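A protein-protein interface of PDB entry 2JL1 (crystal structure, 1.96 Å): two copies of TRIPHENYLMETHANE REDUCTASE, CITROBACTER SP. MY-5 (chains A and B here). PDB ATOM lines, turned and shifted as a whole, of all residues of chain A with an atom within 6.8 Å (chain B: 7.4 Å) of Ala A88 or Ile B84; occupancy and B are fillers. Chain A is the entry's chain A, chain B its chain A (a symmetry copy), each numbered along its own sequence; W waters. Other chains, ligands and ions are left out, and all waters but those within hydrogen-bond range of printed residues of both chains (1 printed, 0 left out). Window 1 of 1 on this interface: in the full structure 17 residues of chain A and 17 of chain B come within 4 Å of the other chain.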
ATOM      1  N   PHE A  72     -18.722  -5.563 -10.852  1.00  0.00           N
ATOM      2  CA  PHE A  72     -19.027  -4.161 -10.756  1.00  0.00           C
ATOM      3  C   PHE A  72     -18.845  -3.621 -12.191  1.00  0.00           C
ATOM      4  O   PHE A  72     -17.729  -3.501 -12.675  1.00  0.00           O
ATOM      5  CB  PHE A  72     -18.042  -3.547  -9.751  1.00  0.00           C
ATOM      6  CG  PHE A  72     -18.077  -2.039  -9.658  1.00  0.00           C
ATOM      7  CD1 PHE A  72     -19.071  -1.294 -10.301  1.00  0.00           C
ATOM      8  CD2 PHE A  72     -17.117  -1.369  -8.906  1.00  0.00           C
ATOM      9  CE1 PHE A  72     -19.086   0.100 -10.230  1.00  0.00           C
ATOM     10  CE2 PHE A  72     -17.146   0.025  -8.809  1.00  0.00           C
ATOM     11  CZ  PHE A  72     -18.137   0.751  -9.504  1.00  0.00           C
ATOM     12  N   LEU A  82     -19.158  13.052 -10.894  1.00  0.00           N
ATOM     13  CA  LEU A  82     -20.238  12.317 -10.235  1.00  0.00           C
ATOM     14  C   LEU A  82     -19.997  10.823 -10.256  1.00  0.00           C
ATOM     15  O   LEU A  82     -20.239  10.133  -9.267  1.00  0.00           O
ATOM     16  CB  LEU A  82     -21.607  12.621 -10.878  1.00  0.00           C
ATOM     17  CG  LEU A  82     -22.738  11.683 -10.436  1.00  0.00           C
ATOM     18  CD1 LEU A  82     -22.995  11.857  -8.916  1.00  0.00           C
ATOM     19  CD2 LEU A  82     -24.027  11.983 -11.246  1.00  0.00           C
ATOM     20  N   LEU A  83     -19.542  10.307 -11.393  1.00  0.00           N
ATOM     21  CA  LEU A  83     -19.236   8.884 -11.512  1.00  0.00           C
ATOM     22  C   LEU A  83     -18.222   8.370 -10.457  1.00  0.00           C
ATOM     23  O   LEU A  83     -18.350   7.260  -9.967  1.00  0.00           O
ATOM     24  CB  LEU A  83     -18.745   8.588 -12.930  1.00  0.00           C
ATOM     25  CG  LEU A  83     -18.792   7.144 -13.379  1.00  0.00           C
ATOM     26  CD1 LEU A  83     -20.224   6.589 -13.200  1.00  0.00           C
ATOM     27  CD2 LEU A  83     -18.346   7.073 -14.815  1.00  0.00           C
ATOM     28  N   ILE A  84     -17.228   9.182 -10.126  1.00  0.00           N
ATOM     29  CA  ILE A  84     -16.259   8.847  -9.062  1.00  0.00           C
ATOM     30  C   ILE A  84     -16.949   8.629  -7.712  1.00  0.00           C
ATOM     31  O   ILE A  84     -16.690   7.614  -7.028  1.00  0.00           O
ATOM     32  CB  ILE A  84     -15.147   9.910  -9.004  1.00  0.00           C
ATOM     33  CG1 ILE A  84     -14.287   9.749 -10.281  1.00  0.00           C
ATOM     34  CG2 ILE A  84     -14.361   9.870  -7.656  1.00  0.00           C
ATOM     35  CD1 ILE A  84     -12.866  10.055 -10.136  1.00  0.00           C
ATOM     36  N   VAL A  85     -17.823   9.572  -7.337  1.00  0.00           N
ATOM     37  CA  VAL A  85     -18.658   9.444  -6.123  1.00  0.00           C
ATOM     38  C   VAL A  85     -19.487   8.168  -6.163  1.00  0.00           C
ATOM     39  O   VAL A  85     -19.529   7.432  -5.188  1.00  0.00           O
ATOM     40  CB  VAL A  85     -19.612  10.675  -5.882  1.00  0.00           C
ATOM     41  CG1 VAL A  85     -20.389  10.511  -4.574  1.00  0.00           C
ATOM     42  CG2 VAL A  85     -18.819  11.963  -5.818  1.00  0.00           C
ATOM     43  N   GLN A  86     -20.155   7.909  -7.289  1.00  0.00           N
ATOM     44  CA  GLN A  86     -21.002   6.709  -7.401  1.00  0.00           C
ATOM     45  C   GLN A  86     -20.169   5.449  -7.236  1.00  0.00           C
ATOM     46  O   GLN A  86     -20.514   4.545  -6.459  1.00  0.00           O
ATOM     47  CB  GLN A  86     -21.728   6.684  -8.746  1.00  0.00           C
ATOM     48  CG  GLN A  86     -22.836   7.741  -8.860  1.00  0.00           C
ATOM     49  CD  GLN A  86     -23.484   7.745 -10.223  1.00  0.00           C
ATOM     50  OE1 GLN A  86     -22.935   7.203 -11.186  1.00  0.00           O
ATOM     51  NE2 GLN A  86     -24.660   8.354 -10.321  1.00  0.00           N
ATOM     52  N   HIS A  87     -19.053   5.405  -7.958  1.00  0.00           N
ATOM     53  CA  HIS A  87     -18.135   4.275  -7.877  1.00  0.00           C
ATOM     54  C   HIS A  87     -17.572   4.127  -6.471  1.00  0.00           C
ATOM     55  O   HIS A  87     -17.437   3.024  -5.986  1.00  0.00           O
ATOM     56  CB  HIS A  87     -17.006   4.423  -8.906  1.00  0.00           C
ATOM     57  CG  HIS A  87     -17.423   4.127 -10.322  1.00  0.00           C
ATOM     58  ND1 HIS A  87     -16.516   3.826 -11.311  1.00  0.00           N
ATOM     59  CD2 HIS A  87     -18.647   4.078 -10.908  1.00  0.00           C
ATOM     60  CE1 HIS A  87     -17.160   3.598 -12.446  1.00  0.00           C
ATOM     61  NE2 HIS A  87     -18.454   3.735 -12.224  1.00  0.00           N
ATOM     62  N   ALA A  88     -17.240   5.231  -5.808  1.00  0.00           N
ATOM     63  CA  ALA A  88     -16.729   5.140  -4.437  1.00  0.00           C
ATOM     64  C   ALA A  88     -17.770   4.539  -3.484  1.00  0.00           C
ATOM     65  O   ALA A  88     -17.417   3.744  -2.617  1.00  0.00           O
ATOM     66  CB  ALA A  88     -16.240   6.484  -3.920  1.00  0.00           C
ATOM     67  N   ASN A  89     -19.041   4.921  -3.655  1.00  0.00           N
ATOM     68  CA  ASN A  89     -20.151   4.325  -2.899  1.00  0.00           C
ATOM     69  C   ASN A  89     -20.257   2.826  -3.139  1.00  0.00           C
ATOM     70  O   ASN A  89     -20.504   2.066  -2.196  1.00  0.00           O
ATOM     71  CB  ASN A  89     -21.505   4.942  -3.278  1.00  0.00           C
ATOM     72  CG  ASN A  89     -21.670   6.373  -2.827  1.00  0.00           C
ATOM     73  OD1 ASN A  89     -21.022   6.851  -1.886  1.00  0.00           O
ATOM     74  ND2 ASN A  89     -22.593   7.080  -3.505  1.00  0.00           N
ATOM     75  N   VAL A  90     -20.101   2.397  -4.399  1.00  0.00           N
ATOM     76  CA  VAL A  90     -20.168   0.965  -4.729  1.00  0.00           C
ATOM     77  C   VAL A  90     -19.088   0.171  -3.987  1.00  0.00           C
ATOM     78  O   VAL A  90     -19.376  -0.839  -3.332  1.00  0.00           O
ATOM     79  CB  VAL A  90     -20.065   0.714  -6.259  1.00  0.00           C
ATOM     80  CG1 VAL A  90     -19.918  -0.769  -6.556  1.00  0.00           C
ATOM     81  CG2 VAL A  90     -21.313   1.260  -6.960  1.00  0.00           C
ATOM     82  N   VAL A  91     -17.852   0.636  -4.093  1.00  0.00           N
ATOM     83  CA  VAL A  91     -16.694  -0.022  -3.482  1.00  0.00           C
ATOM     84  C   VAL A  91     -16.869  -0.096  -1.965  1.00  0.00           C
ATOM     85  O   VAL A  91     -16.601  -1.149  -1.366  1.00  0.00           O
ATOM     86  CB  VAL A  91     -15.382   0.713  -3.861  1.00  0.00           C
ATOM     87  CG1 VAL A  91     -14.177   0.101  -3.165  1.00  0.00           C
ATOM     88  CG2 VAL A  91     -15.186   0.685  -5.363  1.00  0.00           C
ATOM     89  N   LYS A  92     -17.336   0.990  -1.343  1.00  0.00           N
ATOM     90  CA  LYS A  92     -17.523   0.962   0.126  1.00  0.00           C
ATOM     91  C   LYS A  92     -18.614  -0.024   0.523  1.00  0.00           C
ATOM     92  O   LYS A  92     -18.452  -0.769   1.489  1.00  0.00           O
ATOM     93  CB  LYS A  92     -17.853   2.330   0.706  1.00  0.00           C
ATOM     94  CG  LYS A  92     -17.697   2.367   2.235  1.00  0.00           C
ATOM     95  CD  LYS A  92     -18.231   3.629   2.816  1.00  0.00           C
ATOM     96  CE  LYS A  92     -18.112   3.598   4.338  1.00  0.00           C
ATOM     97  NZ  LYS A  92     -19.242   2.811   4.888  1.00  0.00           N
ATOM     98  N   ALA A  93     -19.722  -0.022  -0.223  1.00  0.00           N
ATOM     99  CA  ALA A  93     -20.815  -0.983   0.002  1.00  0.00           C
ATOM    100  C   ALA A  93     -20.323  -2.432  -0.125  1.00  0.00           C
ATOM    101  O   ALA A  93     -20.610  -3.283   0.744  1.00  0.00           O
ATOM    102  CB  ALA A  93     -21.969  -0.718  -0.935  1.00  0.00           C
ATOM    103  N   ALA A 123      -9.118   5.858 -10.819  1.00  0.00           N
ATOM    104  CA  ALA A 123      -9.553   6.226  -9.461  1.00  0.00           C
ATOM    105  C   ALA A 123     -10.317   5.063  -8.828  1.00  0.00           C
ATOM    106  O   ALA A 123     -10.129   4.744  -7.638  1.00  0.00           O
ATOM    107  CB  ALA A 123     -10.419   7.516  -9.486  1.00  0.00           C
ATOM    108  N   THR A 124     -11.168   4.410  -9.630  1.00  0.00           N
ATOM    109  CA  THR A 124     -12.003   3.299  -9.158  1.00  0.00           C
ATOM    110  C   THR A 124     -11.165   2.059  -8.850  1.00  0.00           C
ATOM    111  O   THR A 124     -11.367   1.396  -7.817  1.00  0.00           O
ATOM    112  CB  THR A 124     -13.134   2.989 -10.176  1.00  0.00           C
ATOM    113  OG1 THR A 124     -13.900   4.189 -10.359  1.00  0.00           O
ATOM    114  CG2 THR A 124     -14.041   1.853  -9.649  1.00  0.00           C
ATOM    115  N   TYR A 126      -7.964   2.105  -7.891  1.00  0.00           N
ATOM    116  CA  TYR A 126      -7.332   2.432  -6.610  1.00  0.00           C
ATOM    117  C   TYR A 126      -8.270   2.338  -5.425  1.00  0.00           C
ATOM    118  O   TYR A 126      -7.852   1.885  -4.351  1.00  0.00           O
ATOM    119  CB  TYR A 126      -6.632   3.794  -6.652  1.00  0.00           C
ATOM    120  CG  TYR A 126      -5.317   3.732  -7.341  1.00  0.00           C
ATOM    121  CD1 TYR A 126      -4.245   3.020  -6.768  1.00  0.00           C
ATOM    122  CD2 TYR A 126      -5.117   4.354  -8.564  1.00  0.00           C
ATOM    123  CE1 TYR A 126      -3.015   2.943  -7.406  1.00  0.00           C
ATOM    124  CE2 TYR A 126      -3.879   4.293  -9.200  1.00  0.00           C
ATOM    125  CZ  TYR A 126      -2.841   3.578  -8.612  1.00  0.00           C
ATOM    126  OH  TYR A 126      -1.622   3.505  -9.227  1.00  0.00           O
ATOM    127  N   ALA A 127      -9.531   2.744  -5.601  1.00  0.00           N
ATOM    128  CA  ALA A 127     -10.545   2.547  -4.566  1.00  0.00           C
ATOM    129  C   ALA A 127     -10.722   1.066  -4.199  1.00  0.00           C
ATOM    130  O   ALA A 127     -10.746   0.705  -3.026  1.00  0.00           O
ATOM    131  CB  ALA A 127     -11.897   3.167  -4.979  1.00  0.00           C
ATOM    132  N   ILE A 128     -10.842   0.210  -5.211  1.00  0.00           N
ATOM    133  CA  ILE A 128     -10.979  -1.236  -4.977  1.00  0.00           C
ATOM    134  C   ILE A 128      -9.748  -1.815  -4.267  1.00  0.00           C
ATOM    135  O   ILE A 128      -9.877  -2.697  -3.396  1.00  0.00           O
ATOM    136  CB  ILE A 128     -11.263  -1.997  -6.303  1.00  0.00           C
ATOM    137  CG1 ILE A 128     -12.676  -1.661  -6.779  1.00  0.00           C
ATOM    138  CG2 ILE A 128     -11.038  -3.529  -6.116  1.00  0.00           C
ATOM    139  CD1 ILE A 128     -12.977  -1.966  -8.307  1.00  0.00           C
ATOM    140  N   THR A 130      -7.944  -0.343  -1.998  1.00  0.00           N
ATOM    141  CA  THR A 130      -8.060  -0.014  -0.553  1.00  0.00           C
ATOM    142  C   THR A 130      -8.893  -0.996   0.263  1.00  0.00           C
ATOM    143  O   THR A 130      -8.796  -1.028   1.502  1.00  0.00           O
ATOM    144  CB  THR A 130      -8.623   1.412  -0.303  1.00  0.00           C
ATOM    145  OG1 THR A 130     -10.057   1.424  -0.495  1.00  0.00           O
ATOM    146  CG2 THR A 130      -7.950   2.405  -1.201  1.00  0.00           C
ATOM    147  N   ASP B  79     -10.123   4.515   8.313  1.00  0.00           N
ATOM    148  CA  ASP B  79     -10.765   3.637   7.346  1.00  0.00           C
ATOM    149  C   ASP B  79     -10.481   4.207   5.950  1.00  0.00           C
ATOM    150  O   ASP B  79     -11.050   5.220   5.549  1.00  0.00           O
ATOM    151  CB  ASP B  79     -12.264   3.582   7.662  1.00  0.00           C
ATOM    152  CG  ASP B  79     -13.061   2.688   6.719  1.00  0.00           C
ATOM    153  OD1 ASP B  79     -12.579   2.272   5.628  1.00  0.00           O
ATOM    154  OD2 ASP B  79     -14.226   2.418   7.084  1.00  0.00           O
ATOM    155  N   ASN B  80      -9.570   3.557   5.235  1.00  0.00           N
ATOM    156  CA  ASN B  80      -9.148   3.985   3.899  1.00  0.00           C
ATOM    157  C   ASN B  80     -10.279   3.985   2.874  1.00  0.00           C
ATOM    158  O   ASN B  80     -10.337   4.862   2.037  1.00  0.00           O
ATOM    159  CB  ASN B  80      -8.011   3.105   3.407  1.00  0.00           C
ATOM    160  CG  ASN B  80      -6.725   3.323   4.196  1.00  0.00           C
ATOM    161  OD1 ASN B  80      -6.481   4.418   4.705  1.00  0.00           O
ATOM    162  ND2 ASN B  80      -5.904   2.290   4.293  1.00  0.00           N
ATOM    163  N   THR B  81     -11.166   2.997   2.944  1.00  0.00           N
ATOM    164  CA  THR B  81     -12.272   2.934   1.989  1.00  0.00           C
ATOM    165  C   THR B  81     -13.284   4.051   2.237  1.00  0.00           C
ATOM    166  O   THR B  81     -13.818   4.630   1.289  1.00  0.00           O
ATOM    167  CB  THR B  81     -12.916   1.566   1.995  1.00  0.00           C
ATOM    168  OG1 THR B  81     -11.903   0.587   1.726  1.00  0.00           O
ATOM    169  CG2 THR B  81     -14.045   1.464   0.937  1.00  0.00           C
ATOM    170  N   LEU B  82     -13.570   4.345   3.506  1.00  0.00           N
ATOM    171  CA  LEU B  82     -14.388   5.510   3.844  1.00  0.00           C
ATOM    172  C   LEU B  82     -13.738   6.802   3.397  1.00  0.00           C
ATOM    173  O   LEU B  82     -14.408   7.699   2.887  1.00  0.00           O
ATOM    174  CB  LEU B  82     -14.677   5.582   5.357  1.00  0.00           C
ATOM    175  CG  LEU B  82     -15.278   6.913   5.826  1.00  0.00           C
ATOM    176  CD1 LEU B  82     -16.672   7.113   5.172  1.00  0.00           C
ATOM    177  CD2 LEU B  82     -15.394   6.931   7.373  1.00  0.00           C
ATOM    178  N   LEU B  83     -12.431   6.919   3.608  1.00  0.00           N
ATOM    179  CA  LEU B  83     -11.696   8.105   3.180  1.00  0.00           C
ATOM    180  C   LEU B  83     -11.841   8.422   1.669  1.00  0.00           C
ATOM    181  O   LEU B  83     -11.915   9.578   1.285  1.00  0.00           O
ATOM    182  CB  LEU B  83     -10.224   7.956   3.567  1.00  0.00           C
ATOM    183  CG  LEU B  83      -9.398   9.223   3.608  1.00  0.00           C
ATOM    184  CD1 LEU B  83     -10.076  10.257   4.537  1.00  0.00           C
ATOM    185  CD2 LEU B  83      -8.011   8.879   4.081  1.00  0.00           C
ATOM    186  N   ILE B  84     -11.877   7.393   0.835  1.00  0.00           N
ATOM    187  CA  ILE B  84     -12.114   7.562  -0.614  1.00  0.00           C
ATOM    188  C   ILE B  84     -13.457   8.241  -0.896  1.00  0.00           C
ATOM    189  O   ILE B  84     -13.520   9.212  -1.682  1.00  0.00           O
ATOM    190  CB  ILE B  84     -11.959   6.212  -1.338  1.00  0.00           C
ATOM    191  CG1 ILE B  84     -10.458   5.837  -1.301  1.00  0.00           C
ATOM    192  CG2 ILE B  84     -12.614   6.222  -2.754  1.00  0.00           C
ATOM    193  CD1 ILE B  84      -9.957   5.095  -2.455  1.00  0.00           C
ATOM    194  N   VAL B  85     -14.519   7.737  -0.255  1.00  0.00           N
ATOM    195  CA  VAL B  85     -15.859   8.358  -0.326  1.00  0.00           C
ATOM    196  C   VAL B  85     -15.811   9.811   0.125  1.00  0.00           C
ATOM    197  O   VAL B  85     -16.353  10.679  -0.544  1.00  0.00           O
ATOM    198  CB  VAL B  85     -16.954   7.592   0.509  1.00  0.00           C
ATOM    199  CG1 VAL B  85     -18.327   8.243   0.330  1.00  0.00           C
ATOM    200  CG2 VAL B  85     -17.043   6.145   0.076  1.00  0.00           C
ATOM    201  N   GLN B  86     -15.170  10.077   1.265  1.00  0.00           N
ATOM    202  CA  GLN B  86     -15.101  11.453   1.786  1.00  0.00           C
ATOM    203  C   GLN B  86     -14.379  12.360   0.804  1.00  0.00           C
ATOM    204  O   GLN B  86     -14.860  13.452   0.460  1.00  0.00           O
ATOM    205  CB  GLN B  86     -14.396  11.482   3.142  1.00  0.00           C
ATOM    206  CG  GLN B  86     -15.229  10.866   4.275  1.00  0.00           C
ATOM    207  CD  GLN B  86     -14.479  10.839   5.585  1.00  0.00           C
ATOM    208  OE1 GLN B  86     -13.254  10.978   5.615  1.00  0.00           O
ATOM    209  NE2 GLN B  86     -15.206  10.662   6.682  1.00  0.00           N
ATOM    210  N   HIS B  87     -13.226  11.890   0.334  1.00  0.00           N
ATOM    211  CA  HIS B  87     -12.439  12.633  -0.642  1.00  0.00           C
ATOM    212  C   HIS B  87     -13.216  12.829  -1.936  1.00  0.00           C
ATOM    213  O   HIS B  87     -13.155  13.888  -2.525  1.00  0.00           O
ATOM    214  CB  HIS B  87     -11.103  11.926  -0.908  1.00  0.00           C
ATOM    215  CG  HIS B  87     -10.093  12.087   0.196  1.00  0.00           C
ATOM    216  ND1 HIS B  87      -8.748  11.878   0.003  1.00  0.00           N
ATOM    217  CD2 HIS B  87     -10.233  12.446   1.499  1.00  0.00           C
ATOM    218  CE1 HIS B  87      -8.098  12.105   1.134  1.00  0.00           C
ATOM    219  NE2 HIS B  87      -8.976  12.460   2.053  1.00  0.00           N
ATOM    220  N   ALA B  88     -13.950  11.817  -2.388  1.00  0.00           N
ATOM    221  CA  ALA B  88     -14.745  11.972  -3.610  1.00  0.00           C
ATOM    222  C   ALA B  88     -15.822  13.054  -3.451  1.00  0.00           C
ATOM    223  O   ALA B  88     -16.057  13.822  -4.380  1.00  0.00           O
ATOM    224  CB  ALA B  88     -15.366  10.658  -4.058  1.00  0.00           C
ATOM    225  N   ASN B  89     -16.461  13.104  -2.277  1.00  0.00           N
ATOM    226  CA  ASN B  89     -17.418  14.170  -1.947  1.00  0.00           C
ATOM    227  C   ASN B  89     -16.770  15.546  -1.992  1.00  0.00           C
ATOM    228  O   ASN B  89     -17.381  16.500  -2.484  1.00  0.00           O
ATOM    229  CB  ASN B  89     -18.015  13.995  -0.543  1.00  0.00           C
ATOM    230  CG  ASN B  89     -18.945  12.812  -0.418  1.00  0.00           C
ATOM    231  OD1 ASN B  89     -19.524  12.318  -1.396  1.00  0.00           O
ATOM    232  ND2 ASN B  89     -19.117  12.354   0.835  1.00  0.00           N
ATOM    233  N   VAL B  90     -15.546  15.661  -1.456  1.00  0.00           N
ATOM    234  CA  VAL B  90     -14.830  16.946  -1.467  1.00  0.00           C
ATOM    235  C   VAL B  90     -14.599  17.443  -2.897  1.00  0.00           C
ATOM    236  O   VAL B  90     -14.917  18.591  -3.234  1.00  0.00           O
ATOM    237  CB  VAL B  90     -13.481  16.868  -0.699  1.00  0.00           C
ATOM    238  CG1 VAL B  90     -12.665  18.132  -0.908  1.00  0.00           C
ATOM    239  CG2 VAL B  90     -13.746  16.665   0.795  1.00  0.00           C
ATOM    240  N   VAL B  91     -14.047  16.573  -3.731  1.00  0.00           N
ATOM    241  CA  VAL B  91     -13.719  16.894  -5.122  1.00  0.00           C
ATOM    242  C   VAL B  91     -14.983  17.294  -5.883  1.00  0.00           C
ATOM    243  O   VAL B  91     -14.961  18.281  -6.635  1.00  0.00           O
ATOM    244  CB  VAL B  91     -13.005  15.699  -5.807  1.00  0.00           C
ATOM    245  CG1 VAL B  91     -12.736  15.977  -7.278  1.00  0.00           C
ATOM    246  CG2 VAL B  91     -11.708  15.389  -5.089  1.00  0.00           C
ATOM    247  N   HIS B 119      -2.884   4.265  -1.833  1.00  0.00           N
ATOM    248  CA  HIS B 119      -3.962   4.024  -2.783  1.00  0.00           C
ATOM    249  C   HIS B 119      -5.043   5.100  -2.710  1.00  0.00           C
ATOM    250  O   HIS B 119      -5.626   5.478  -3.742  1.00  0.00           O
ATOM    251  CB  HIS B 119      -4.510   2.608  -2.615  1.00  0.00           C
ATOM    252  CG  HIS B 119      -3.534   1.559  -3.037  1.00  0.00           C
ATOM    253  ND1 HIS B 119      -3.495   0.295  -2.490  1.00  0.00           N
ATOM    254  CD2 HIS B 119      -2.513   1.622  -3.918  1.00  0.00           C
ATOM    255  CE1 HIS B 119      -2.527  -0.394  -3.064  1.00  0.00           C
ATOM    256  NE2 HIS B 119      -1.905   0.395  -3.922  1.00  0.00           N
ATOM    257  N   VAL B 120      -5.318   5.567  -1.492  1.00  0.00           N
ATOM    258  CA  VAL B 120      -6.304   6.619  -1.263  1.00  0.00           C
ATOM    259  C   VAL B 120      -5.840   7.899  -1.947  1.00  0.00           C
ATOM    260  O   VAL B 120      -6.635   8.601  -2.575  1.00  0.00           O
ATOM    261  CB  VAL B 120      -6.456   6.946   0.242  1.00  0.00           C
ATOM    262  CG1 VAL B 120      -7.360   8.185   0.427  1.00  0.00           C
ATOM    263  CG2 VAL B 120      -7.048   5.758   1.019  1.00  0.00           C
ATOM    264  N   HIS B 121      -4.556   8.222  -1.779  1.00  0.00           N
ATOM    265  CA  HIS B 121      -4.016   9.458  -2.339  1.00  0.00           C
ATOM    266  C   HIS B 121      -4.028   9.440  -3.857  1.00  0.00           C
ATOM    267  O   HIS B 121      -4.379  10.439  -4.506  1.00  0.00           O
ATOM    268  CB  HIS B 121      -2.618   9.739  -1.765  1.00  0.00           C
ATOM    269  CG  HIS B 121      -2.653  10.130  -0.325  1.00  0.00           C
ATOM    270  ND1 HIS B 121      -3.395  11.204   0.137  1.00  0.00           N
ATOM    271  CD2 HIS B 121      -2.102   9.555   0.767  1.00  0.00           C
ATOM    272  CE1 HIS B 121      -3.276  11.280   1.453  1.00  0.00           C
ATOM    273  NE2 HIS B 121      -2.485  10.300   1.857  1.00  0.00           N
ATOM    274  N   LEU B 122      -3.688   8.289  -4.433  1.00  0.00           N
ATOM    275  CA  LEU B 122      -3.702   8.157  -5.914  1.00  0.00           C
ATOM    276  C   LEU B 122      -5.143   8.209  -6.470  1.00  0.00           C
ATOM    277  O   LEU B 122      -5.397   8.861  -7.498  1.00  0.00           O
ATOM    278  CB  LEU B 122      -2.988   6.882  -6.342  1.00  0.00           C
ATOM    279  CG  LEU B 122      -1.447   6.926  -6.242  1.00  0.00           C
ATOM    280  CD1 LEU B 122      -0.856   5.501  -6.071  1.00  0.00           C
ATOM    281  CD2 LEU B 122      -0.847   7.624  -7.462  1.00  0.00           C
ATOM    282  N   ALA B 123      -6.083   7.563  -5.775  1.00  0.00           N
ATOM    283  CA  ALA B 123      -7.503   7.616  -6.158  1.00  0.00           C
ATOM    284  C   ALA B 123      -7.994   9.064  -6.132  1.00  0.00           C
ATOM    285  O   ALA B 123      -8.731   9.508  -7.035  1.00  0.00           O
ATOM    286  CB  ALA B 123      -8.363   6.718  -5.228  1.00  0.00           C
ATOM    287  N   THR B 124      -7.567   9.813  -5.108  1.00  0.00           N
ATOM    288  CA  THR B 124      -7.985  11.208  -4.922  1.00  0.00           C
ATOM    289  C   THR B 124      -7.379  12.120  -5.988  1.00  0.00           C
ATOM    290  O   THR B 124      -8.073  12.986  -6.551  1.00  0.00           O
ATOM    291  CB  THR B 124      -7.646  11.698  -3.488  1.00  0.00           C
ATOM    292  OG1 THR B 124      -8.300  10.820  -2.559  1.00  0.00           O
ATOM    293  CG2 THR B 124      -8.135  13.150  -3.282  1.00  0.00           C
ATOM    294  N   ALA B 127      -9.357  11.513  -9.057  1.00  0.00           N
ATOM    295  CA  ALA B 127     -10.622  12.228  -8.894  1.00  0.00           C
ATOM    296  C   ALA B 127     -10.497  13.720  -9.234  1.00  0.00           C
ATOM    297  O   ALA B 127     -11.314  14.272  -9.966  1.00  0.00           O
ATOM    298  CB  ALA B 127     -11.192  12.044  -7.472  1.00  0.00           C
HETATM  299  O   HOH W   1      -6.667  -0.352   2.735  1.00  0.00           O
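OG1 of Thr B81 sits at hydrogen-bond distance from OG1 of Thr A130 (3.0 Å).
The side-chain hydroxyl of Thr A130 sits at hydrogen-bond distance from the backbone carbonyl oxygen of Ala A127 (2.7 Å).
The side-chain carboxylate (OD1) of Asp B79 lies within hydrogen-bond range of the backbone NH (N) of Thr B81, at 3.1 Å.
N of Leu B82 lies within hydrogen-bond range of OD1 of Asp B79, 3.1 Å away.
Among the printed residues, pairs that only touch across the chains: Ala A127 with Ile B84 (3.4 Å), Ile A84 with Ala B127 (3.4 Å), Tyr A126 with His B119 (3.5 Å), Ala A123 with Ala B123 (3.6 Å), Thr A130 with Ile B84 (3.6 Å), Tyr A126 with Leu B122 (3.6 Å), Lys A92 with Thr B81 (3.6 Å), Val A85 with Ala B88 (3.6 Å), Ala A88 with Val B85 (3.6 Å), Tyr A126 with Ala B123 (3.7 Å), Thr A130 with His B119 (3.7 Å), Asn A89 with Val B85 (3.8 Å), Val A85 with Asn B89 (3.8 Å), Ala A88 with Ile B84 (3.8 Å), Ile A84 with Ala B88 (3.8 Å), Lys A92 with Leu B82 (3.9 Å) and Lys A92 with Val B85 (3.9 Å).
Of the printed residues of chain B, Ile A84 touches Ala B88 (3.8 Å) and Ala B127 (3.4 Å).
Ala A88 touches just these residues of chain B: Ile B84 (3.8 Å) and Val B85 (3.6 Å).
Thr A124 touches none of the printed residues of chain B.
Of the printed residues of chain B, Tyr A126 touches His B119 (3.5 Å), Leu B122 (3.6 Å) and Ala B123 (3.7 Å).
Asn B80 touches none of the printed residues of chain A.
Ile B84 touches just these residues of chain A: Ala A88, Ala A127 and Thr A130.
Printed residues of chain A within 4 Å of His B119: Tyr A126 and Thr A130.
The nearest residue of chain A that does not touch Ile B84 is Tyr A126 (4.3 Å).
Printed residues of chain B that touch a printed residue of chain A: Thr B81, Leu B82, Ile B84, Val B85, Ala B88, Asn B89, His B119, Leu B122, Ala B123 and Ala B127.
Hydrophobic or aromatic side chains of chain B that line the printed part of chain A: Leu B82, Ile B84, Val B85, Ala B88, His B119, Leu B122, Ala B123 and Ala B127.
Among the printed residues, no Asp or Glu carboxylate lies within 4 Å of a Lys or Arg side-chain nitrogen of the other chain.
Ile A84 touches Ala B88, and with the chains exchanged Ala A88 touches Ile B84.
Ile A84 touches Ala B127, and with the chains exchanged Ala A127 touches Ile B84.
Val A85 touches Ala B88, and with the chains exchanged Ala A88 touches Val B85.
Ala A123 touches its own counterpart, Ala B123.
13 positions are printed for both chains.
Of the 18 pairs that touch across the chains among the printed residues, 9 have their exchanged pair printed and touching as well.
Water W1 lies within hydrogen-bond range of the backbone carbonyl oxygen of Thr A130 and the side-chain amide nitrogen of Asn B80.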
